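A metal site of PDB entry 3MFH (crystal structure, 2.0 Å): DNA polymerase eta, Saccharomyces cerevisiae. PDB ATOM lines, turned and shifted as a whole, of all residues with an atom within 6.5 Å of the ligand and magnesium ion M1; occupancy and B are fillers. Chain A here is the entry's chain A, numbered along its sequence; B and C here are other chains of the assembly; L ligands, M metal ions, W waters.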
ATOM      1  N   ASP A  37     -37.053  20.473 -34.930  1.00  0.00           N
ATOM      2  CA  ASP A  37     -35.874  20.970 -34.264  1.00  0.00           C
ATOM      3  C   ASP A  37     -34.620  20.490 -35.014  1.00  0.00           C
ATOM      4  O   ASP A  37     -34.449  19.304 -35.237  1.00  0.00           O
ATOM      5  CB  ASP A  37     -35.865  20.463 -32.847  1.00  0.00           C
ATOM      6  CG  ASP A  37     -34.734  21.014 -32.028  1.00  0.00           C
ATOM      7  OD1 ASP A  37     -33.571  20.720 -32.345  1.00  0.00           O
ATOM      8  OD2 ASP A  37     -34.997  21.729 -31.034  1.00  0.00           O
ATOM      9  N   MET A  38     -33.758  21.427 -35.376  1.00  0.00           N
ATOM     10  CA  MET A  38     -32.546  21.137 -36.141  1.00  0.00           C
ATOM     11  C   MET A  38     -31.597  20.309 -35.293  1.00  0.00           C
ATOM     12  O   MET A  38     -31.385  20.603 -34.127  1.00  0.00           O
ATOM     13  CB  MET A  38     -31.847  22.432 -36.529  1.00  0.00           C
ATOM     14  CG  MET A  38     -32.686  23.346 -37.387  1.00  0.00           C
ATOM     15  SD  MET A  38     -32.603  22.774 -39.084  1.00  0.00           S
ATOM     16  CE  MET A  38     -33.752  23.903 -39.851  1.00  0.00           C
ATOM     17  N   ASN A  39     -31.057  19.247 -35.884  1.00  0.00           N
ATOM     18  CA  ASN A  39     -30.147  18.359 -35.185  1.00  0.00           C
ATOM     19  C   ASN A  39     -28.790  19.086 -35.017  1.00  0.00           C
ATOM     20  O   ASN A  39     -28.272  19.634 -35.982  1.00  0.00           O
ATOM     21  CB  ASN A  39     -29.931  17.050 -36.001  1.00  0.00           C
ATOM     22  CG  ASN A  39     -31.167  16.156 -36.067  1.00  0.00           C
ATOM     23  OD1 ASN A  39     -31.357  15.448 -37.061  1.00  0.00           O
ATOM     24  ND2 ASN A  39     -31.995  16.150 -35.016  1.00  0.00           N
ATOM     25  N   ALA A  40     -28.244  19.094 -33.795  1.00  0.00           N
ATOM     26  CA  ALA A  40     -26.891  19.577 -33.541  1.00  0.00           C
ATOM     27  C   ALA A  40     -26.638  20.887 -34.290  1.00  0.00           C
ATOM     28  O   ALA A  40     -25.660  21.023 -35.019  1.00  0.00           O
ATOM     29  CB  ALA A  40     -25.838  18.481 -33.980  1.00  0.00           C
ATOM     30  N   PHE A  41     -27.521  21.854 -34.117  1.00  0.00           N
ATOM     31  CA  PHE A  41     -27.606  22.948 -35.076  1.00  0.00           C
ATOM     32  C   PHE A  41     -26.282  23.683 -35.366  1.00  0.00           C
ATOM     33  O   PHE A  41     -25.872  23.734 -36.502  1.00  0.00           O
ATOM     34  CB  PHE A  41     -28.711  23.923 -34.688  1.00  0.00           C
ATOM     35  CG  PHE A  41     -28.940  24.990 -35.690  1.00  0.00           C
ATOM     36  CD1 PHE A  41     -29.080  24.685 -37.051  1.00  0.00           C
ATOM     37  CD2 PHE A  41     -29.020  26.320 -35.304  1.00  0.00           C
ATOM     38  CE1 PHE A  41     -29.276  25.719 -37.999  1.00  0.00           C
ATOM     39  CE2 PHE A  41     -29.225  27.324 -36.231  1.00  0.00           C
ATOM     40  CZ  PHE A  41     -29.346  27.020 -37.579  1.00  0.00           C
ATOM     41  N   PHE A  42     -25.620  24.265 -34.369  1.00  0.00           N
ATOM     42  CA  PHE A  42     -24.440  25.076 -34.657  1.00  0.00           C
ATOM     43  C   PHE A  42     -23.346  24.201 -35.276  1.00  0.00           C
ATOM     44  O   PHE A  42     -22.574  24.687 -36.085  1.00  0.00           O
ATOM     45  CB  PHE A  42     -23.892  25.774 -33.425  1.00  0.00           C
ATOM     46  CG  PHE A  42     -24.762  26.886 -32.881  1.00  0.00           C
ATOM     47  CD1 PHE A  42     -26.064  27.100 -33.332  1.00  0.00           C
ATOM     48  CD2 PHE A  42     -24.287  27.689 -31.862  1.00  0.00           C
ATOM     49  CE1 PHE A  42     -26.851  28.090 -32.802  1.00  0.00           C
ATOM     50  CE2 PHE A  42     -25.070  28.700 -31.325  1.00  0.00           C
ATOM     51  CZ  PHE A  42     -26.359  28.882 -31.791  1.00  0.00           C
ATOM     52  N   ALA A  43     -23.293  22.925 -34.901  1.00  0.00           N
ATOM     53  CA  ALA A  43     -22.279  22.006 -35.440  1.00  0.00           C
ATOM     54  C   ALA A  43     -22.567  21.687 -36.893  1.00  0.00           C
ATOM     55  O   ALA A  43     -21.661  21.632 -37.694  1.00  0.00           O
ATOM     56  CB  ALA A  43     -22.197  20.736 -34.641  1.00  0.00           C
ATOM     57  N   GLN A  62     -17.277  27.621 -28.138  1.00  0.00           N
ATOM     58  CA  GLN A  62     -17.417  29.000 -27.727  1.00  0.00           C
ATOM     59  C   GLN A  62     -16.530  29.197 -26.510  1.00  0.00           C
ATOM     60  O   GLN A  62     -16.876  28.778 -25.393  1.00  0.00           O
ATOM     61  CB  GLN A  62     -18.872  29.344 -27.389  1.00  0.00           C
ATOM     62  CG  GLN A  62     -19.123  30.815 -27.133  1.00  0.00           C
ATOM     63  CD  GLN A  62     -20.578  31.123 -26.831  1.00  0.00           C
ATOM     64  OE1 GLN A  62     -21.323  31.557 -27.727  1.00  0.00           O
ATOM     65  NE2 GLN A  62     -20.992  30.876 -25.579  1.00  0.00           N
ATOM     66  N   ILE A  67     -20.411  24.126 -27.483  1.00  0.00           N
ATOM     67  CA  ILE A  67     -21.759  24.722 -27.518  1.00  0.00           C
ATOM     68  C   ILE A  67     -22.689  23.836 -28.348  1.00  0.00           C
ATOM     69  O   ILE A  67     -23.914  23.838 -28.143  1.00  0.00           O
ATOM     70  CB  ILE A  67     -21.703  26.212 -27.991  1.00  0.00           C
ATOM     71  CG1 ILE A  67     -23.016  26.927 -27.827  1.00  0.00           C
ATOM     72  CG2 ILE A  67     -21.314  26.345 -29.465  1.00  0.00           C
ATOM     73  CD1 ILE A  67     -22.897  28.450 -28.040  1.00  0.00           C
ATOM     74  N   ALA A  68     -22.107  23.065 -29.273  1.00  0.00           N
ATOM     75  CA  ALA A  68     -22.858  22.057 -30.030  1.00  0.00           C
ATOM     76  C   ALA A  68     -21.984  20.885 -30.448  1.00  0.00           C
ATOM     77  O   ALA A  68     -20.806  21.039 -30.803  1.00  0.00           O
ATOM     78  CB  ALA A  68     -23.545  22.701 -31.263  1.00  0.00           C
ATOM     79  N   VAL A  69     -22.560  19.689 -30.403  1.00  0.00           N
ATOM     80  CA  VAL A  69     -21.824  18.472 -30.717  1.00  0.00           C
ATOM     81  C   VAL A  69     -22.555  17.733 -31.815  1.00  0.00           C
ATOM     82  O   VAL A  69     -23.679  17.263 -31.605  1.00  0.00           O
ATOM     83  CB  VAL A  69     -21.640  17.575 -29.453  1.00  0.00           C
ATOM     84  CG1 VAL A  69     -22.912  17.420 -28.726  1.00  0.00           C
ATOM     85  CG2 VAL A  69     -21.057  16.182 -29.815  1.00  0.00           C
ATOM     86  N   TYR A  71     -23.592  14.726 -34.359  1.00  0.00           N
ATOM     87  CA  TYR A  71     -23.941  13.333 -34.061  1.00  0.00           C
ATOM     88  C   TYR A  71     -22.770  12.365 -34.282  1.00  0.00           C
ATOM     89  O   TYR A  71     -22.667  11.352 -33.563  1.00  0.00           O
ATOM     90  CB  TYR A  71     -25.224  12.900 -34.771  1.00  0.00           C
ATOM     91  CG  TYR A  71     -26.431  13.456 -34.006  1.00  0.00           C
ATOM     92  CD1 TYR A  71     -26.812  14.783 -34.145  1.00  0.00           C
ATOM     93  CD2 TYR A  71     -27.092  12.691 -33.061  1.00  0.00           C
ATOM     94  CE1 TYR A  71     -27.880  15.312 -33.437  1.00  0.00           C
ATOM     95  CE2 TYR A  71     -28.171  13.204 -32.353  1.00  0.00           C
ATOM     96  CZ  TYR A  71     -28.553  14.519 -32.542  1.00  0.00           C
ATOM     97  OH  TYR A  71     -29.592  15.043 -31.821  1.00  0.00           O
ATOM     98  N   ARG A  74     -20.920  12.631 -30.976  1.00  0.00           N
ATOM     99  CA  ARG A  74     -21.653  12.016 -29.861  1.00  0.00           C
ATOM    100  C   ARG A  74     -21.405  10.502 -29.735  1.00  0.00           C
ATOM    101  O   ARG A  74     -21.562   9.920 -28.639  1.00  0.00           O
ATOM    102  CB  ARG A  74     -23.152  12.281 -29.976  1.00  0.00           C
ATOM    103  CG  ARG A  74     -23.542  13.766 -29.954  1.00  0.00           C
ATOM    104  CD  ARG A  74     -25.057  13.958 -30.006  1.00  0.00           C
ATOM    105  NE  ARG A  74     -25.353  15.337 -30.374  1.00  0.00           N
ATOM    106  CZ  ARG A  74     -26.465  15.987 -30.079  1.00  0.00           C
ATOM    107  NH1 ARG A  74     -27.415  15.399 -29.371  1.00  0.00           N
ATOM    108  NH2 ARG A  74     -26.599  17.266 -30.450  1.00  0.00           N
ATOM    109  N   ARG A  80     -22.649  18.230 -24.914  1.00  0.00           N
ATOM    110  CA  ARG A  80     -22.678  19.692 -24.875  1.00  0.00           C
ATOM    111  C   ARG A  80     -22.203  20.095 -23.505  1.00  0.00           C
ATOM    112  O   ARG A  80     -22.499  19.446 -22.510  1.00  0.00           O
ATOM    113  CB  ARG A  80     -24.097  20.247 -25.106  1.00  0.00           C
ATOM    114  CG  ARG A  80     -24.196  21.293 -26.214  1.00  0.00           C
ATOM    115  CD  ARG A  80     -25.660  21.759 -26.424  1.00  0.00           C
ATOM    116  NE  ARG A  80     -26.124  22.352 -25.190  1.00  0.00           N
ATOM    117  CZ  ARG A  80     -25.759  23.549 -24.751  1.00  0.00           C
ATOM    118  NH1 ARG A  80     -24.968  24.353 -25.467  1.00  0.00           N
ATOM    119  NH2 ARG A  80     -26.207  23.957 -23.565  1.00  0.00           N
ATOM    120  N   MET A  81     -21.443  21.178 -23.476  1.00  0.00           N
ATOM    121  CA  MET A  81     -20.911  21.769 -22.246  1.00  0.00           C
ATOM    122  C   MET A  81     -19.740  21.002 -21.634  1.00  0.00           C
ATOM    123  O   MET A  81     -19.205  21.427 -20.592  1.00  0.00           O
ATOM    124  CB  MET A  81     -22.010  22.095 -21.224  1.00  0.00           C
ATOM    125  CG  MET A  81     -22.773  23.374 -21.551  1.00  0.00           C
ATOM    126  SD  MET A  81     -21.611  24.761 -21.682  1.00  0.00           S
ATOM    127  CE  MET A  81     -21.176  25.037 -19.960  1.00  0.00           C
ATOM    128  N   LEU A 135     -22.922  35.182 -33.272  1.00  0.00           N
ATOM    129  CA  LEU A 135     -23.831  34.074 -33.578  1.00  0.00           C
ATOM    130  C   LEU A 135     -24.518  34.270 -34.922  1.00  0.00           C
ATOM    131  O   LEU A 135     -25.387  33.477 -35.292  1.00  0.00           O
ATOM    132  CB  LEU A 135     -24.879  33.922 -32.478  1.00  0.00           C
ATOM    133  CG  LEU A 135     -24.365  33.668 -31.064  1.00  0.00           C
ATOM    134  CD1 LEU A 135     -25.541  33.525 -30.121  1.00  0.00           C
ATOM    135  CD2 LEU A 135     -23.431  32.424 -31.013  1.00  0.00           C
ATOM    136  N   SER A 160     -37.477  29.290 -31.436  1.00  0.00           N
ATOM    137  CA  SER A 160     -36.125  29.645 -30.986  1.00  0.00           C
ATOM    138  C   SER A 160     -35.214  29.505 -32.200  1.00  0.00           C
ATOM    139  O   SER A 160     -35.693  29.245 -33.304  1.00  0.00           O
ATOM    140  CB  SER A 160     -35.656  28.760 -29.806  1.00  0.00           C
ATOM    141  OG  SER A 160     -35.460  27.417 -30.205  1.00  0.00           O
ATOM    142  N   ILE A 161     -33.918  29.729 -32.028  1.00  0.00           N
ATOM    143  CA  ILE A 161     -33.024  29.786 -33.187  1.00  0.00           C
ATOM    144  C   ILE A 161     -33.127  28.521 -34.079  1.00  0.00           C
ATOM    145  O   ILE A 161     -33.008  28.621 -35.300  1.00  0.00           O
ATOM    146  CB  ILE A 161     -31.571  30.068 -32.815  1.00  0.00           C
ATOM    147  CG1 ILE A 161     -30.803  30.485 -34.078  1.00  0.00           C
ATOM    148  CG2 ILE A 161     -30.921  28.836 -32.098  1.00  0.00           C
ATOM    149  CD1 ILE A 161     -29.580  31.282 -33.803  1.00  0.00           C
ATOM    150  N   ASP A 162     -33.432  27.372 -33.500  1.00  0.00           N
ATOM    151  CA  ASP A 162     -33.464  26.145 -34.303  1.00  0.00           C
ATOM    152  C   ASP A 162     -34.757  25.320 -34.229  1.00  0.00           C
ATOM    153  O   ASP A 162     -34.791  24.166 -34.704  1.00  0.00           O
ATOM    154  CB  ASP A 162     -32.203  25.299 -34.001  1.00  0.00           C
ATOM    155  CG  ASP A 162     -32.424  24.240 -32.957  1.00  0.00           C
ATOM    156  OD1 ASP A 162     -31.783  23.175 -33.106  1.00  0.00           O
ATOM    157  OD2 ASP A 162     -33.185  24.429 -31.960  1.00  0.00           O
ATOM    158  N   GLU A 163     -35.801  25.917 -33.670  1.00  0.00           N
ATOM    159  CA  GLU A 163     -37.115  25.282 -33.526  1.00  0.00           C
ATOM    160  C   GLU A 163     -38.172  26.060 -34.285  1.00  0.00           C
ATOM    161  O   GLU A 163     -38.185  27.301 -34.224  1.00  0.00           O
ATOM    162  CB  GLU A 163     -37.590  25.296 -32.081  1.00  0.00           C
ATOM    163  CG  GLU A 163     -36.745  24.566 -31.063  1.00  0.00           C
ATOM    164  CD  GLU A 163     -37.348  24.741 -29.671  1.00  0.00           C
ATOM    165  OE1 GLU A 163     -36.540  25.044 -28.765  1.00  0.00           O
ATOM    166  OE2 GLU A 163     -38.601  24.632 -29.488  1.00  0.00           O
ATOM    167  N   SER A 268     -35.113  16.587 -36.262  1.00  0.00           N
ATOM    168  CA  SER A 268     -36.027  15.695 -35.585  1.00  0.00           C
ATOM    169  C   SER A 268     -37.349  16.427 -35.476  1.00  0.00           C
ATOM    170  O   SER A 268     -37.393  17.664 -35.449  1.00  0.00           O
ATOM    171  CB  SER A 268     -35.474  15.335 -34.225  1.00  0.00           C
ATOM    172  OG  SER A 268     -34.464  14.348 -34.425  1.00  0.00           O
ATOM    173  N   ASN A 283     -38.031  15.616 -29.482  1.00  0.00           N
ATOM    174  CA  ASN A 283     -36.825  15.309 -28.711  1.00  0.00           C
ATOM    175  C   ASN A 283     -36.708  13.817 -28.373  1.00  0.00           C
ATOM    176  O   ASN A 283     -35.740  13.387 -27.806  1.00  0.00           O
ATOM    177  CB  ASN A 283     -36.827  16.147 -27.428  1.00  0.00           C
ATOM    178  CG  ASN A 283     -35.425  16.483 -26.932  1.00  0.00           C
ATOM    179  OD1 ASN A 283     -34.559  16.982 -27.688  1.00  0.00           O
ATOM    180  ND2 ASN A 283     -35.202  16.231 -25.660  1.00  0.00           N
ATOM    181  N   LYS A 286     -33.496  11.140 -32.033  1.00  0.00           N
ATOM    182  CA  LYS A 286     -32.593  11.956 -32.818  1.00  0.00           C
ATOM    183  C   LYS A 286     -31.364  11.116 -33.216  1.00  0.00           C
ATOM    184  O   LYS A 286     -30.983  10.214 -32.472  1.00  0.00           O
ATOM    185  CB  LYS A 286     -32.028  13.113 -31.979  1.00  0.00           C
ATOM    186  CG  LYS A 286     -32.921  13.888 -31.011  1.00  0.00           C
ATOM    187  CD  LYS A 286     -32.015  14.319 -29.809  1.00  0.00           C
ATOM    188  CE  LYS A 286     -32.645  15.378 -29.030  1.00  0.00           C
ATOM    189  NZ  LYS A 286     -31.717  16.007 -28.093  1.00  0.00           N
ATOM    190  N   PRO A 287     -30.712  11.452 -34.342  1.00  0.00           N
ATOM    191  CA  PRO A 287     -31.066  12.514 -35.303  1.00  0.00           C
ATOM    192  C   PRO A 287     -31.974  12.002 -36.401  1.00  0.00           C
ATOM    193  O   PRO A 287     -32.277  10.814 -36.460  1.00  0.00           O
ATOM    194  CB  PRO A 287     -29.721  12.859 -35.930  1.00  0.00           C
ATOM    195  CG  PRO A 287     -29.041  11.477 -36.048  1.00  0.00           C
ATOM    196  CD  PRO A 287     -29.548  10.676 -34.820  1.00  0.00           C
ATOM    197  O5'  DT B   4     -21.463  27.667 -15.077  1.00  0.00           O
ATOM    198  C5'  DT B   4     -21.614  27.416 -16.485  1.00  0.00           C
ATOM    199  C4'  DT B   4     -20.819  28.404 -17.339  1.00  0.00           C
ATOM    200  O4'  DT B   4     -20.889  27.998 -18.734  1.00  0.00           O
ATOM    201  C3'  DT B   4     -21.289  29.868 -17.328  1.00  0.00           C
ATOM    202  O3'  DT B   4     -20.170  30.717 -17.507  1.00  0.00           O
ATOM    203  C2'  DT B   4     -22.254  29.907 -18.515  1.00  0.00           C
ATOM    204  C1'  DT B   4     -21.532  28.979 -19.514  1.00  0.00           C
ATOM    205  N1   DT B   4     -22.370  28.248 -20.536  1.00  0.00           N
ATOM    206  C2   DT B   4     -23.508  27.576 -20.147  1.00  0.00           C
ATOM    207  O2   DT B   4     -23.918  27.549 -18.995  1.00  0.00           O
ATOM    208  N3   DT B   4     -24.171  26.913 -21.160  1.00  0.00           N
ATOM    209  C4   DT B   4     -23.828  26.863 -22.501  1.00  0.00           C
ATOM    210  O4   DT B   4     -24.501  26.230 -23.308  1.00  0.00           O
ATOM    211  C5   DT B   4     -22.604  27.577 -22.858  1.00  0.00           C
ATOM    212  C7   DT B   4     -22.130  27.587 -24.289  1.00  0.00           C
ATOM    213  C6   DT B   4     -21.941  28.216 -21.873  1.00  0.00           C
ATOM    214  P    DT B   5     -20.277  32.297 -17.743  1.00  0.00           P
ATOM    215  OP1  DT B   5     -18.914  32.785 -17.510  1.00  0.00           O
ATOM    216  OP2  DT B   5     -21.450  32.832 -17.038  1.00  0.00           O
ATOM    217  O5'  DT B   5     -20.614  32.477 -19.323  1.00  0.00           O
ATOM    218  C5'  DT B   5     -19.599  32.238 -20.290  1.00  0.00           C
ATOM    219  C4'  DT B   5     -20.132  32.446 -21.683  1.00  0.00           C
ATOM    220  O4'  DT B   5     -21.287  31.606 -21.914  1.00  0.00           O
ATOM    221  C3'  DT B   5     -20.591  33.878 -21.985  1.00  0.00           C
ATOM    222  O3'  DT B   5     -20.089  34.201 -23.246  1.00  0.00           O
ATOM    223  C2'  DT B   5     -22.122  33.787 -21.903  1.00  0.00           C
ATOM    224  C1'  DT B   5     -22.324  32.384 -22.483  1.00  0.00           C
ATOM    225  N1   DT B   5     -23.543  31.585 -22.150  1.00  0.00           N
ATOM    226  C2   DT B   5     -24.090  30.769 -23.123  1.00  0.00           C
ATOM    227  O2   DT B   5     -23.668  30.718 -24.256  1.00  0.00           O
ATOM    228  N3   DT B   5     -25.152  30.014 -22.704  1.00  0.00           N
ATOM    229  C4   DT B   5     -25.707  29.995 -21.426  1.00  0.00           C
ATOM    230  O4   DT B   5     -26.656  29.288 -21.131  1.00  0.00           O
ATOM    231  C5   DT B   5     -25.087  30.848 -20.441  1.00  0.00           C
ATOM    232  C7   DT B   5     -25.630  30.892 -19.033  1.00  0.00           C
ATOM    233  C6   DT B   5     -24.036  31.598 -20.852  1.00  0.00           C
ATOM    234  P    DG B   6     -20.211  35.660 -23.868  1.00  0.00           P
ATOM    235  OP1  DG B   6     -19.081  35.808 -24.809  1.00  0.00           O
ATOM    236  OP2  DG B   6     -20.463  36.640 -22.790  1.00  0.00           O
ATOM    237  O5'  DG B   6     -21.534  35.556 -24.723  1.00  0.00           O
ATOM    238  C5'  DG B   6     -21.492  34.847 -25.983  1.00  0.00           C
ATOM    239  C4'  DG B   6     -22.897  34.770 -26.550  1.00  0.00           C
ATOM    240  O4'  DG B   6     -23.695  33.937 -25.650  1.00  0.00           O
ATOM    241  C3'  DG B   6     -23.602  36.132 -26.644  1.00  0.00           C
ATOM    242  O3'  DG B   6     -24.245  36.255 -27.893  1.00  0.00           O
ATOM    243  C2'  DG B   6     -24.570  36.049 -25.476  1.00  0.00           C
ATOM    244  C1'  DG B   6     -24.922  34.575 -25.491  1.00  0.00           C
ATOM    245  N9   DG B   6     -25.626  34.119 -24.295  1.00  0.00           N
ATOM    246  C8   DG B   6     -25.572  34.617 -23.010  1.00  0.00           C
ATOM    247  N7   DG B   6     -26.377  34.022 -22.188  1.00  0.00           N
ATOM    248  C5   DG B   6     -27.007  33.081 -22.991  1.00  0.00           C
ATOM    249  C6   DG B   6     -28.008  32.125 -22.672  1.00  0.00           C
ATOM    250  O6   DG B   6     -28.515  31.946 -21.577  1.00  0.00           O
ATOM    251  N1   DG B   6     -28.402  31.354 -23.779  1.00  0.00           N
ATOM    252  C2   DG B   6     -27.871  31.495 -25.053  1.00  0.00           C
ATOM    253  N2   DG B   6     -28.325  30.680 -26.024  1.00  0.00           N
ATOM    254  N3   DG B   6     -26.934  32.385 -25.349  1.00  0.00           N
ATOM    255  C4   DG B   6     -26.558  33.131 -24.285  1.00  0.00           C
ATOM    256  N1  DOC C  11     -31.652  27.635 -24.385  1.00  0.00           N
ATOM    257  C2  DOC C  11     -30.767  28.710 -24.539  1.00  0.00           C
ATOM    258  N3  DOC C  11     -30.401  29.427 -23.468  1.00  0.00           N
ATOM    259  C4  DOC C  11     -30.893  29.110 -22.242  1.00  0.00           C
ATOM    260  C5  DOC C  11     -31.767  28.039 -22.081  1.00  0.00           C
ATOM    261  C6  DOC C  11     -32.152  27.323 -23.194  1.00  0.00           C
ATOM    262  O2  DOC C  11     -30.333  28.992 -25.685  1.00  0.00           O
ATOM    263  N4  DOC C  11     -30.526  29.814 -21.165  1.00  0.00           N
ATOM    264  C1' DOC C  11     -32.019  26.907 -25.598  1.00  0.00           C
ATOM    265  C2' DOC C  11     -31.843  25.390 -25.419  1.00  0.00           C
ATOM    266  C3' DOC C  11     -32.887  24.857 -26.355  1.00  0.00           C
ATOM    267  C4' DOC C  11     -33.941  25.963 -26.447  1.00  0.00           C
ATOM    268  O4' DOC C  11     -33.388  27.174 -25.924  1.00  0.00           O
ATOM    269  C5' DOC C  11     -35.202  25.555 -25.698  1.00  0.00           C
ATOM    270  O5' DOC C  11     -34.893  24.980 -24.410  1.00  0.00           O
ATOM    271  P   DOC C  11     -36.121  24.399 -23.555  1.00  0.00           P
ATOM    272  OP1 DOC C  11     -36.836  23.405 -24.411  1.00  0.00           O
ATOM    273  OP2 DOC C  11     -35.586  23.944 -22.232  1.00  0.00           O
HETATM  274  P1  LIG L   1     -30.204  18.498 -30.831  1.00  0.00           P
HETATM  275  O1  LIG L   1     -31.379  19.385 -31.086  1.00  0.00           O
HETATM  276  O2  LIG L   1     -30.176  17.674 -29.572  1.00  0.00           O
HETATM  277  O3  LIG L   1     -29.833  17.657 -32.032  1.00  0.00           O
HETATM  278  P2  LIG L   1     -28.819  21.040 -30.772  1.00  0.00           P
HETATM  279  O4  LIG L   1     -29.602  21.471 -31.978  1.00  0.00           O
HETATM  280  O5  LIG L   1     -27.303  21.316 -30.778  1.00  0.00           O
HETATM  281  O6  LIG L   1     -28.939  19.458 -30.546  1.00  0.00           O
HETATM  282  P3  LIG L   1     -30.686  22.556 -29.137  1.00  0.00           P
HETATM  283  O7  LIG L   1     -31.748  22.174 -30.132  1.00  0.00           O
HETATM  284  O8  LIG L   1     -30.987  22.486 -27.681  1.00  0.00           O
HETATM  285  O9  LIG L   1     -29.368  21.627 -29.371  1.00  0.00           O
HETATM  286  O10 LIG L   1     -30.194  24.061 -29.432  1.00  0.00           O
HETATM  287  C1  LIG L   1     -29.972  24.567 -30.739  1.00  0.00           C
HETATM  288  C2  LIG L   1     -28.651  25.328 -30.801  1.00  0.00           C
HETATM  289  O11 LIG L   1     -28.697  26.415 -29.871  1.00  0.00           O
HETATM  290  C3  LIG L   1     -27.412  24.507 -30.434  1.00  0.00           C
HETATM  291  O12 LIG L   1     -26.842  23.848 -31.583  1.00  0.00           O
HETATM  292  C4  LIG L   1     -26.464  25.510 -29.807  1.00  0.00           C
HETATM  293  C5  LIG L   1     -27.431  26.529 -29.226  1.00  0.00           C
HETATM  294  N1  LIG L   1     -27.633  26.375 -27.762  1.00  0.00           N
HETATM  295  C6  LIG L   1     -28.372  25.446 -27.108  1.00  0.00           C
HETATM  296  N2  LIG L   1     -28.318  25.627 -25.753  1.00  0.00           N
HETATM  297  C7  LIG L   1     -27.542  26.676 -25.535  1.00  0.00           C
HETATM  298  C8  LIG L   1     -27.078  27.403 -24.341  1.00  0.00           C
HETATM  299  N3  LIG L   1     -27.460  27.007 -23.101  1.00  0.00           N
HETATM  300  N4  LIG L   1     -26.245  28.452 -24.550  1.00  0.00           N
HETATM  301  C9  LIG L   1     -25.867  28.827 -25.783  1.00  0.00           C
HETATM  302  N5  LIG L   1     -26.248  28.214 -26.900  1.00  0.00           N
HETATM  303  C10 LIG L   1     -27.069  27.157 -26.840  1.00  0.00           C
HETATM  304 MG    MG M   1     -31.652  21.254 -32.044  1.00  0.00          MG
HETATM  305 MG    MG M   2     -34.050  23.735 -28.986  1.00  0.00          MG
HETATM  306  O   HOH W   1     -30.315  28.623 -28.549  1.00  0.00           O
HETATM  307  O   HOH W   2     -33.454  21.363 -27.221  1.00  0.00           O
HETATM  308  O   HOH W   3     -26.294  30.657 -28.547  1.00  0.00           O
HETATM  309  O   HOH W   4     -33.422  19.226 -29.211  1.00  0.00           O
HETATM  310  O   HOH W   5     -26.474  25.537 -20.509  1.00  0.00           O
HETATM  311  O   HOH W   6     -32.891  17.858 -32.784  1.00  0.00           O
HETATM  312  O   HOH W   7     -29.501  20.483 -25.947  1.00  0.00           O
HETATM  313  O   HOH W   8     -29.028  24.758 -21.650  1.00  0.00           O
HETATM  314  O   HOH W   9     -28.884  17.987 -27.415  1.00  0.00           O
HETATM  315  O   HOH W  10     -25.316  19.790 -29.600  1.00  0.00           O
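N2 of DG 6 of chain B sits close to N5 of the ligand.
CA of Asn 39 touches O3 of the ligand (3.2 Å).
Ile 67 touches the ligand (O to C4, 3.5 Å).
CB of Ala 68 touches O12 of the ligand, at 3.5 Å.
Ile 161 touches the ligand (CG2 to O11, 3.97 Å).
DOC 11 of chain C touches the ligand.
Hydrophobic or aromatic side chains that line the ligand: Phe 41, Phe 42, Ile 67, Ala 68, Tyr 71 and Ile 161.
18 residues have an atom within 4 Å of the ligand: Asp 37, Met 38, Asn 39, Ala 40, Phe 41, Phe 42, Ile 67, Ala 68, Tyr 71, Arg 74, Arg 80, Ile 161, Asp 162, Lys 286, DT 4 of chain B, DT 5 of chain B, DG 6 of chain B and DOC 11 of chain C.
Within 4 Å of magnesium ion M1: Asp 37, Met 38 and Asp 162.
Magnesium ion M1 is bound by OD1 of Asp 37 (2.0 Å), O4 of the ligand (2.1 Å), O1 of the ligand (2.1 Å), O7 of the ligand (2.1 Å), O of Met 38 (2.2 Å) and OD1 of Asp 162 (2.2 Å).
Magnesium ion M1 has six donor atoms within binding distance.
The side-chain hydroxyl of Tyr 71 is in hydrogen-bond range of an oxygen (O3) of the ligand (2.6 Å).
O4 of DT 5 of chain B is in hydrogen-bond range of a nitrogen (N3) of the ligand (3.1 Å).
The side-chain amino group of Lys 286 is in salt-bridge range of an oxygen (O2) of the ligand (2.7 Å).
O3 of the ligand is in hydrogen-bond range of N of Ala 40 (2.8 Å).
N of Phe 41 is in hydrogen-bond range of O12 of the ligand (3.3 Å).
O4 of DT 4 of chain B lies close to a nitrogen (N3) of the ligand, 3.1 Å away.
O12 of the ligand sits at hydrogen-bond distance from N of Phe 42 (3.1 Å).
The guanidinium group (NH1) of Arg 74 is in salt-bridge range of an oxygen (O2) of the ligand.
The guanidinium group (NH2) of Arg 80 sits close to a nitrogen (N2) of the ligand.
The backbone NH of Asp 37 lies within hydrogen-bond range of the backbone carbonyl oxygen of Ser 268, at 2.9 Å.
The side-chain amide nitrogen (NE2) of Gln 62 lies within hydrogen-bond range of O2 of DT 5 of chain B, 3.0 Å away.
NZ of Lys 286 sits close to OD1 of Asn 283 (3.0 Å).
O4 of DT 4 of chain B sits at hydrogen-bond distance from the guanidinium group of Arg 80 (2.9 Å).
N2 of DG 6 of chain B sits close to O2 of DOC 11 of chain C (2.6 Å).
The guanidinium group of Arg 74 is in hydrogen-bond range of the backbone carbonyl oxygen of Val 69, 2.8 Å away.
The side-chain amide nitrogen of Asn 39 sits at hydrogen-bond distance from the side-chain hydroxyl of Ser 268 (3.1 Å).
The guanidinium group of Arg 80 lies within hydrogen-bond range of the backbone carbonyl oxygen of Ile 67 (2.9 Å).
Water W6 lies within hydrogen-bond range of ND2 of Asn 39 (2.9 Å), O3 of the ligand (3.2 Å) and O of Asp 37 (3.2 Å).
Water W10 lies within hydrogen-bond range of an oxygen (O5) of the ligand, the backbone NH of Val 69 and the guanidinium group of Arg 74.
Water W4 lies within hydrogen-bond range of OD1 of Asn 283 and OD2 of Asp 37.
Water W3 lies within hydrogen-bond range of N5 of the ligand (2.9 Å) and N2 of DG 6 of chain B (3.2 Å).
Water W1 bridges O2 of DOC 11 of chain C and an oxygen (O11) of the ligand.
Water W5 lies within hydrogen-bond range of N3 of DT 4 of chain B, a nitrogen (N3) of the ligand and the guanidinium group (NH2) of Arg 80.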
